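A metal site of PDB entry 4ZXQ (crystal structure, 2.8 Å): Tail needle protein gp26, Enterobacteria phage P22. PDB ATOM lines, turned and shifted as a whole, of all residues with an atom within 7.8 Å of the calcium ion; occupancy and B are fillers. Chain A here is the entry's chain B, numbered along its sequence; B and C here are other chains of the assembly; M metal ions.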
ATOM      1  N   ALA A  63      -3.292 -32.763 -10.572  1.00  0.00           N
ATOM      2  CA  ALA A  63      -3.086 -31.766 -11.610  1.00  0.00           C
ATOM      3  C   ALA A  63      -1.628 -31.754 -12.084  1.00  0.00           C
ATOM      4  O   ALA A  63      -1.357 -31.660 -13.285  1.00  0.00           O
ATOM      5  CB  ALA A  63      -3.491 -30.391 -11.110  1.00  0.00           C
ATOM      6  N   GLN A  64      -0.690 -31.873 -11.140  1.00  0.00           N
ATOM      7  CA  GLN A  64       0.723 -31.853 -11.493  1.00  0.00           C
ATOM      8  C   GLN A  64       1.161 -33.083 -12.303  1.00  0.00           C
ATOM      9  O   GLN A  64       1.868 -32.945 -13.309  1.00  0.00           O
ATOM     10  CB  GLN A  64       1.600 -31.767 -10.241  1.00  0.00           C
ATOM     11  CG  GLN A  64       1.457 -30.491  -9.452  1.00  0.00           C
ATOM     12  CD  GLN A  64       2.579 -30.321  -8.438  1.00  0.00           C
ATOM     13  OE1 GLN A  64       3.087 -31.301  -7.891  1.00  0.00           O
ATOM     14  NE2 GLN A  64       2.988 -29.086  -8.193  1.00  0.00           N
ATOM     15  N   LYS A  66      -0.769 -35.025 -14.100  1.00  0.00           N
ATOM     16  CA  LYS A  66      -1.445 -34.926 -15.387  1.00  0.00           C
ATOM     17  C   LYS A  66      -0.684 -33.966 -16.295  1.00  0.00           C
ATOM     18  O   LYS A  66      -0.507 -34.211 -17.498  1.00  0.00           O
ATOM     19  CB  LYS A  66      -2.891 -34.470 -15.207  1.00  0.00           C
ATOM     20  CG  LYS A  66      -3.781 -34.690 -16.416  1.00  0.00           C
ATOM     21  CD  LYS A  66      -3.823 -36.161 -16.787  1.00  0.00           C
ATOM     22  CE  LYS A  66      -4.710 -36.414 -18.000  1.00  0.00           C
ATOM     23  NZ  LYS A  66      -4.609 -37.831 -18.469  1.00  0.00           N
ATOM     24  N   ASN A  67      -0.208 -32.863 -15.700  1.00  0.00           N
ATOM     25  CA  ASN A  67       0.609 -31.897 -16.422  1.00  0.00           C
ATOM     26  C   ASN A  67       1.906 -32.515 -16.935  1.00  0.00           C
ATOM     27  O   ASN A  67       2.365 -32.186 -18.024  1.00  0.00           O
ATOM     28  CB  ASN A  67       0.926 -30.692 -15.541  1.00  0.00           C
ATOM     29  CG  ASN A  67      -0.215 -29.711 -15.469  1.00  0.00           C
ATOM     30  OD1 ASN A  67      -1.152 -29.766 -16.270  1.00  0.00           O
ATOM     31  ND2 ASN A  67      -0.154 -28.786 -14.512  1.00  0.00           N
ATOM     32  N   ASP A  68       2.495 -33.405 -16.142  1.00  0.00           N
ATOM     33  CA  ASP A  68       3.718 -34.097 -16.542  1.00  0.00           C
ATOM     34  C   ASP A  68       3.487 -34.987 -17.768  1.00  0.00           C
ATOM     35  O   ASP A  68       4.230 -34.926 -18.764  1.00  0.00           O
ATOM     36  CB  ASP A  68       4.272 -34.931 -15.392  1.00  0.00           C
ATOM     37  CG  ASP A  68       4.744 -34.081 -14.230  1.00  0.00           C
ATOM     38  OD1 ASP A  68       4.815 -32.844 -14.384  1.00  0.00           O
ATOM     39  OD2 ASP A  68       5.046 -34.648 -13.157  1.00  0.00           O
ATOM     40  N   GLN A  70       1.098 -34.783 -19.904  1.00  0.00           N
ATOM     41  CA  GLN A  70       0.791 -33.887 -21.007  1.00  0.00           C
ATOM     42  C   GLN A  70       2.071 -33.228 -21.533  1.00  0.00           C
ATOM     43  O   GLN A  70       2.138 -32.856 -22.698  1.00  0.00           O
ATOM     44  CB  GLN A  70      -0.219 -32.824 -20.602  1.00  0.00           C
ATOM     45  CG  GLN A  70      -1.628 -33.351 -20.426  1.00  0.00           C
ATOM     46  CD  GLN A  70      -2.613 -32.256 -20.043  1.00  0.00           C
ATOM     47  OE1 GLN A  70      -2.326 -31.075 -20.180  1.00  0.00           O
ATOM     48  NE2 GLN A  70      -3.785 -32.666 -19.571  1.00  0.00           N
ATOM     49  N   ASP A  71       3.073 -33.097 -20.676  1.00  0.00           N
ATOM     50  CA  ASP A  71       4.352 -32.556 -21.092  1.00  0.00           C
ATOM     51  C   ASP A  71       5.056 -33.538 -22.014  1.00  0.00           C
ATOM     52  O   ASP A  71       5.630 -33.148 -23.032  1.00  0.00           O
ATOM     53  CB  ASP A  71       5.242 -32.234 -19.895  1.00  0.00           C
ATOM     54  CG  ASP A  71       5.211 -30.777 -19.509  1.00  0.00           C
ATOM     55  OD1 ASP A  71       4.240 -30.087 -19.879  1.00  0.00           O
ATOM     56  OD2 ASP A  71       6.164 -30.322 -18.851  1.00  0.00           O
ATOM     57  N   LEU A  74       3.239 -33.502 -25.302  1.00  0.00           N
ATOM     58  CA  LEU A  74       3.508 -32.234 -25.975  1.00  0.00           C
ATOM     59  C   LEU A  74       4.881 -32.230 -26.620  1.00  0.00           C
ATOM     60  O   LEU A  74       5.062 -31.704 -27.715  1.00  0.00           O
ATOM     61  CB  LEU A  74       3.389 -31.053 -25.003  1.00  0.00           C
ATOM     62  CG  LEU A  74       1.980 -30.490 -24.791  1.00  0.00           C
ATOM     63  CD1 LEU A  74       1.972 -29.458 -23.669  1.00  0.00           C
ATOM     64  CD2 LEU A  74       1.456 -29.874 -26.074  1.00  0.00           C
ATOM     65  N   ALA B  63      -7.825 -26.127 -12.527  1.00  0.00           N
ATOM     66  CA  ALA B  63      -6.643 -26.749 -13.133  1.00  0.00           C
ATOM     67  C   ALA B  63      -7.030 -28.057 -13.813  1.00  0.00           C
ATOM     68  O   ALA B  63      -6.562 -28.352 -14.920  1.00  0.00           O
ATOM     69  CB  ALA B  63      -5.571 -26.980 -12.083  1.00  0.00           C
ATOM     70  N   GLN B  64      -7.904 -28.821 -13.158  1.00  0.00           N
ATOM     71  CA  GLN B  64      -8.350 -30.089 -13.721  1.00  0.00           C
ATOM     72  C   GLN B  64      -9.228 -29.900 -14.962  1.00  0.00           C
ATOM     73  O   GLN B  64      -9.087 -30.637 -15.944  1.00  0.00           O
ATOM     74  CB  GLN B  64      -9.120 -30.893 -12.659  1.00  0.00           C
ATOM     75  CG  GLN B  64      -8.258 -31.314 -11.478  1.00  0.00           C
ATOM     76  CD  GLN B  64      -8.909 -32.395 -10.634  1.00  0.00           C
ATOM     77  OE1 GLN B  64     -10.130 -32.444 -10.505  1.00  0.00           O
ATOM     78  NE2 GLN B  64      -8.083 -33.257 -10.055  1.00  0.00           N
ATOM     79  N   LYS B  66      -9.102 -27.371 -17.036  1.00  0.00           N
ATOM     80  CA  LYS B  66      -8.164 -26.958 -18.071  1.00  0.00           C
ATOM     81  C   LYS B  66      -7.420 -28.172 -18.604  1.00  0.00           C
ATOM     82  O   LYS B  66      -7.160 -28.274 -19.801  1.00  0.00           O
ATOM     83  CB  LYS B  66      -7.194 -25.911 -17.549  1.00  0.00           C
ATOM     84  CG  LYS B  66      -6.382 -25.227 -18.643  1.00  0.00           C
ATOM     85  CD  LYS B  66      -6.448 -23.715 -18.555  1.00  0.00           C
ATOM     86  CE  LYS B  66      -7.836 -23.198 -18.918  1.00  0.00           C
ATOM     87  NZ  LYS B  66      -7.836 -21.723 -19.133  1.00  0.00           N
ATOM     88  N   ASN B  67      -7.091 -29.091 -17.697  1.00  0.00           N
ATOM     89  CA  ASN B  67      -6.452 -30.340 -18.111  1.00  0.00           C
ATOM     90  C   ASN B  67      -7.339 -31.133 -19.058  1.00  0.00           C
ATOM     91  O   ASN B  67      -6.847 -31.740 -20.015  1.00  0.00           O
ATOM     92  CB  ASN B  67      -6.111 -31.200 -16.886  1.00  0.00           C
ATOM     93  CG  ASN B  67      -4.850 -30.726 -16.182  1.00  0.00           C
ATOM     94  OD1 ASN B  67      -4.080 -29.945 -16.720  1.00  0.00           O
ATOM     95  ND2 ASN B  67      -4.645 -31.215 -14.955  1.00  0.00           N
ATOM     96  N   ASP B  68      -8.644 -31.123 -18.802  1.00  0.00           N
ATOM     97  CA  ASP B  68      -9.592 -31.821 -19.666  1.00  0.00           C
ATOM     98  C   ASP B  68      -9.648 -31.213 -21.060  1.00  0.00           C
ATOM     99  O   ASP B  68      -9.513 -31.915 -22.070  1.00  0.00           O
ATOM    100  CB  ASP B  68     -10.992 -31.802 -19.032  1.00  0.00           C
ATOM    101  CG  ASP B  68     -11.065 -32.604 -17.749  1.00  0.00           C
ATOM    102  OD1 ASP B  68     -10.098 -33.320 -17.444  1.00  0.00           O
ATOM    103  OD2 ASP B  68     -12.103 -32.521 -17.057  1.00  0.00           O
ATOM    104  N   GLN B  70      -7.460 -29.354 -22.480  1.00  0.00           N
ATOM    105  CA  GLN B  70      -6.150 -29.569 -23.085  1.00  0.00           C
ATOM    106  C   GLN B  70      -5.992 -31.008 -23.560  1.00  0.00           C
ATOM    107  O   GLN B  70      -5.250 -31.262 -24.516  1.00  0.00           O
ATOM    108  CB  GLN B  70      -5.042 -29.206 -22.102  1.00  0.00           C
ATOM    109  CG  GLN B  70      -4.879 -27.712 -21.882  1.00  0.00           C
ATOM    110  CD  GLN B  70      -3.768 -27.373 -20.914  1.00  0.00           C
ATOM    111  OE1 GLN B  70      -3.268 -28.247 -20.203  1.00  0.00           O
ATOM    112  NE2 GLN B  70      -3.371 -26.117 -20.880  1.00  0.00           N
ATOM    113  N   ASP B  71      -6.678 -31.936 -22.921  1.00  0.00           N
ATOM    114  CA  ASP B  71      -6.649 -33.330 -23.352  1.00  0.00           C
ATOM    115  C   ASP B  71      -7.412 -33.474 -24.664  1.00  0.00           C
ATOM    116  O   ASP B  71      -6.957 -34.179 -25.583  1.00  0.00           O
ATOM    117  CB  ASP B  71      -7.249 -34.250 -22.294  1.00  0.00           C
ATOM    118  CG  ASP B  71      -6.186 -34.901 -21.418  1.00  0.00           C
ATOM    119  OD1 ASP B  71      -5.061 -34.355 -21.351  1.00  0.00           O
ATOM    120  OD2 ASP B  71      -6.469 -35.952 -20.812  1.00  0.00           O
ATOM    121  N   LEU B  74      -5.304 -31.988 -27.316  1.00  0.00           N
ATOM    122  CA  LEU B  74      -4.190 -32.880 -27.591  1.00  0.00           C
ATOM    123  C   LEU B  74      -4.613 -34.030 -28.497  1.00  0.00           C
ATOM    124  O   LEU B  74      -3.870 -34.415 -29.392  1.00  0.00           O
ATOM    125  CB  LEU B  74      -3.599 -33.431 -26.292  1.00  0.00           C
ATOM    126  CG  LEU B  74      -2.559 -32.543 -25.601  1.00  0.00           C
ATOM    127  CD1 LEU B  74      -2.192 -33.120 -24.236  1.00  0.00           C
ATOM    128  CD2 LEU B  74      -1.325 -32.380 -26.465  1.00  0.00           C
ATOM    129  N   ALA C  63       0.026 -25.695 -10.734  1.00  0.00           N
ATOM    130  CA  ALA C  63      -0.742 -26.429 -11.736  1.00  0.00           C
ATOM    131  C   ALA C  63      -1.274 -25.458 -12.786  1.00  0.00           C
ATOM    132  O   ALA C  63      -1.214 -25.723 -13.984  1.00  0.00           O
ATOM    133  CB  ALA C  63      -1.892 -27.183 -11.076  1.00  0.00           C
ATOM    134  N   GLN C  64      -1.740 -24.308 -12.307  1.00  0.00           N
ATOM    135  CA  GLN C  64      -2.276 -23.298 -13.209  1.00  0.00           C
ATOM    136  C   GLN C  64      -1.207 -22.642 -14.103  1.00  0.00           C
ATOM    137  O   GLN C  64      -1.457 -22.438 -15.290  1.00  0.00           O
ATOM    138  CB  GLN C  64      -3.038 -22.215 -12.426  1.00  0.00           C
ATOM    139  CG  GLN C  64      -4.293 -22.725 -11.709  1.00  0.00           C
ATOM    140  CD  GLN C  64      -5.236 -21.620 -11.252  1.00  0.00           C
ATOM    141  OE1 GLN C  64      -4.792 -20.516 -10.921  1.00  0.00           O
ATOM    142  NE2 GLN C  64      -6.531 -21.918 -11.210  1.00  0.00           N
ATOM    143  N   LYS C  66       1.481 -23.991 -15.089  1.00  0.00           N
ATOM    144  CA  LYS C  66       1.816 -25.033 -16.058  1.00  0.00           C
ATOM    145  C   LYS C  66       0.744 -25.117 -17.152  1.00  0.00           C
ATOM    146  O   LYS C  66       1.075 -25.229 -18.338  1.00  0.00           O
ATOM    147  CB  LYS C  66       1.959 -26.396 -15.383  1.00  0.00           C
ATOM    148  CG  LYS C  66       2.616 -27.425 -16.275  1.00  0.00           C
ATOM    149  CD  LYS C  66       3.997 -26.935 -16.697  1.00  0.00           C
ATOM    150  CE  LYS C  66       4.693 -27.920 -17.595  1.00  0.00           C
ATOM    151  NZ  LYS C  66       5.971 -27.367 -18.128  1.00  0.00           N
ATOM    152  N   ASN C  67      -0.515 -25.018 -16.758  1.00  0.00           N
ATOM    153  CA  ASN C  67      -1.615 -25.021 -17.720  1.00  0.00           C
ATOM    154  C   ASN C  67      -1.538 -23.848 -18.692  1.00  0.00           C
ATOM    155  O   ASN C  67      -1.843 -24.000 -19.873  1.00  0.00           O
ATOM    156  CB  ASN C  67      -2.965 -25.010 -16.999  1.00  0.00           C
ATOM    157  CG  ASN C  67      -3.372 -26.383 -16.507  1.00  0.00           C
ATOM    158  OD1 ASN C  67      -2.796 -27.398 -16.910  1.00  0.00           O
ATOM    159  ND2 ASN C  67      -4.364 -26.428 -15.628  1.00  0.00           N
ATOM    160  N   ASP C  68      -1.142 -22.681 -18.190  1.00  0.00           N
ATOM    161  CA  ASP C  68      -1.017 -21.505 -19.036  1.00  0.00           C
ATOM    162  C   ASP C  68       0.073 -21.667 -20.083  1.00  0.00           C
ATOM    163  O   ASP C  68      -0.174 -21.482 -21.298  1.00  0.00           O
ATOM    164  CB  ASP C  68      -0.737 -20.267 -18.177  1.00  0.00           C
ATOM    165  CG  ASP C  68      -1.906 -19.908 -17.275  1.00  0.00           C
ATOM    166  OD1 ASP C  68      -2.992 -20.497 -17.443  1.00  0.00           O
ATOM    167  OD2 ASP C  68      -1.741 -19.023 -16.400  1.00  0.00           O
ATOM    168  N   GLN C  70       1.388 -24.387 -21.137  1.00  0.00           N
ATOM    169  CA  GLN C  70       0.962 -25.469 -22.027  1.00  0.00           C
ATOM    170  C   GLN C  70      -0.102 -25.002 -23.007  1.00  0.00           C
ATOM    171  O   GLN C  70      -0.223 -25.545 -24.111  1.00  0.00           O
ATOM    172  CB  GLN C  70       0.437 -26.657 -21.223  1.00  0.00           C
ATOM    173  CG  GLN C  70       1.500 -27.462 -20.500  1.00  0.00           C
ATOM    174  CD  GLN C  70       0.904 -28.624 -19.731  1.00  0.00           C
ATOM    175  OE1 GLN C  70       1.623 -29.471 -19.209  1.00  0.00           O
ATOM    176  NE2 GLN C  70      -0.423 -28.658 -19.659  1.00  0.00           N
ATOM    177  N   ASP C  71      -0.867 -23.989 -22.623  1.00  0.00           N
ATOM    178  CA  ASP C  71      -1.876 -23.414 -23.511  1.00  0.00           C
ATOM    179  C   ASP C  71      -1.186 -22.662 -24.631  1.00  0.00           C
ATOM    180  O   ASP C  71      -1.582 -22.764 -25.807  1.00  0.00           O
ATOM    181  CB  ASP C  71      -2.816 -22.481 -22.746  1.00  0.00           C
ATOM    182  CG  ASP C  71      -4.106 -23.159 -22.339  1.00  0.00           C
ATOM    183  OD1 ASP C  71      -4.137 -24.404 -22.273  1.00  0.00           O
ATOM    184  OD2 ASP C  71      -5.107 -22.443 -22.097  1.00  0.00           O
ATOM    185  N   LEU C  74       0.236 -25.236 -26.963  1.00  0.00           N
ATOM    186  CA  LEU C  74      -0.833 -25.877 -27.735  1.00  0.00           C
ATOM    187  C   LEU C  74      -1.300 -24.983 -28.873  1.00  0.00           C
ATOM    188  O   LEU C  74      -1.534 -25.467 -29.992  1.00  0.00           O
ATOM    189  CB  LEU C  74      -2.016 -26.214 -26.820  1.00  0.00           C
ATOM    190  CG  LEU C  74      -1.920 -27.549 -26.071  1.00  0.00           C
ATOM    191  CD1 LEU C  74      -3.059 -27.684 -25.073  1.00  0.00           C
ATOM    192  CD2 LEU C  74      -1.932 -28.711 -27.056  1.00  0.00           C
HETATM  193 CA    CA M   1      -2.341 -29.416 -18.294  1.00  0.00          CA
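ND2 of Asn 67 of chain A sits close to O of Ala 63 of chain A, at 3.3 Å.
The side-chain amide nitrogen of Asn 67 of chain A lies within hydrogen-bond range of the backbone carbonyl oxygen of Ala 63 of chain C, 3.3 Å away.
The side-chain amide nitrogen (ND2) of Asn 67 of chain B sits close to the backbone carbonyl oxygen (O) of Ala 63 of chain B (3.4 Å).
OE1 of Gln 70 of chain C sits close to OD1 of Asp 71 of chain A, at 2.8 Å.
The backbone carbonyl oxygen (O) of Ala 63 of chain B is in hydrogen-bond range of the side-chain amide nitrogen (ND2) of Asn 67 of chain C (3.0 Å).
NE2 of Gln 70 of chain A is in hydrogen-bond range of OD1 of Asp 71 of chain B (2.8 Å).
The nearest printed residue that does not touch the calcium ion is Lys 66 of chain B (5.2 Å).
The calcium ion is bound by the side-chain amide oxygen (OD1) of Asn 67 of chain A (2.4 Å), the side-chain amide oxygen (OD1) of Asn 67 of chain B (2.4 Å), the side-chain amide oxygen (OE1) of Gln 70 of chain B (2.4 Å), the side-chain amide nitrogen (NE2) of Gln 70 of chain C (2.5 Å), the side-chain amide oxygen (OD1) of Asn 67 of chain C (2.5 Å) and the side-chain amide oxygen (OE1) of Gln 70 of chain A (2.5 Å).
The calcium ion has six donor atoms within binding distance.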
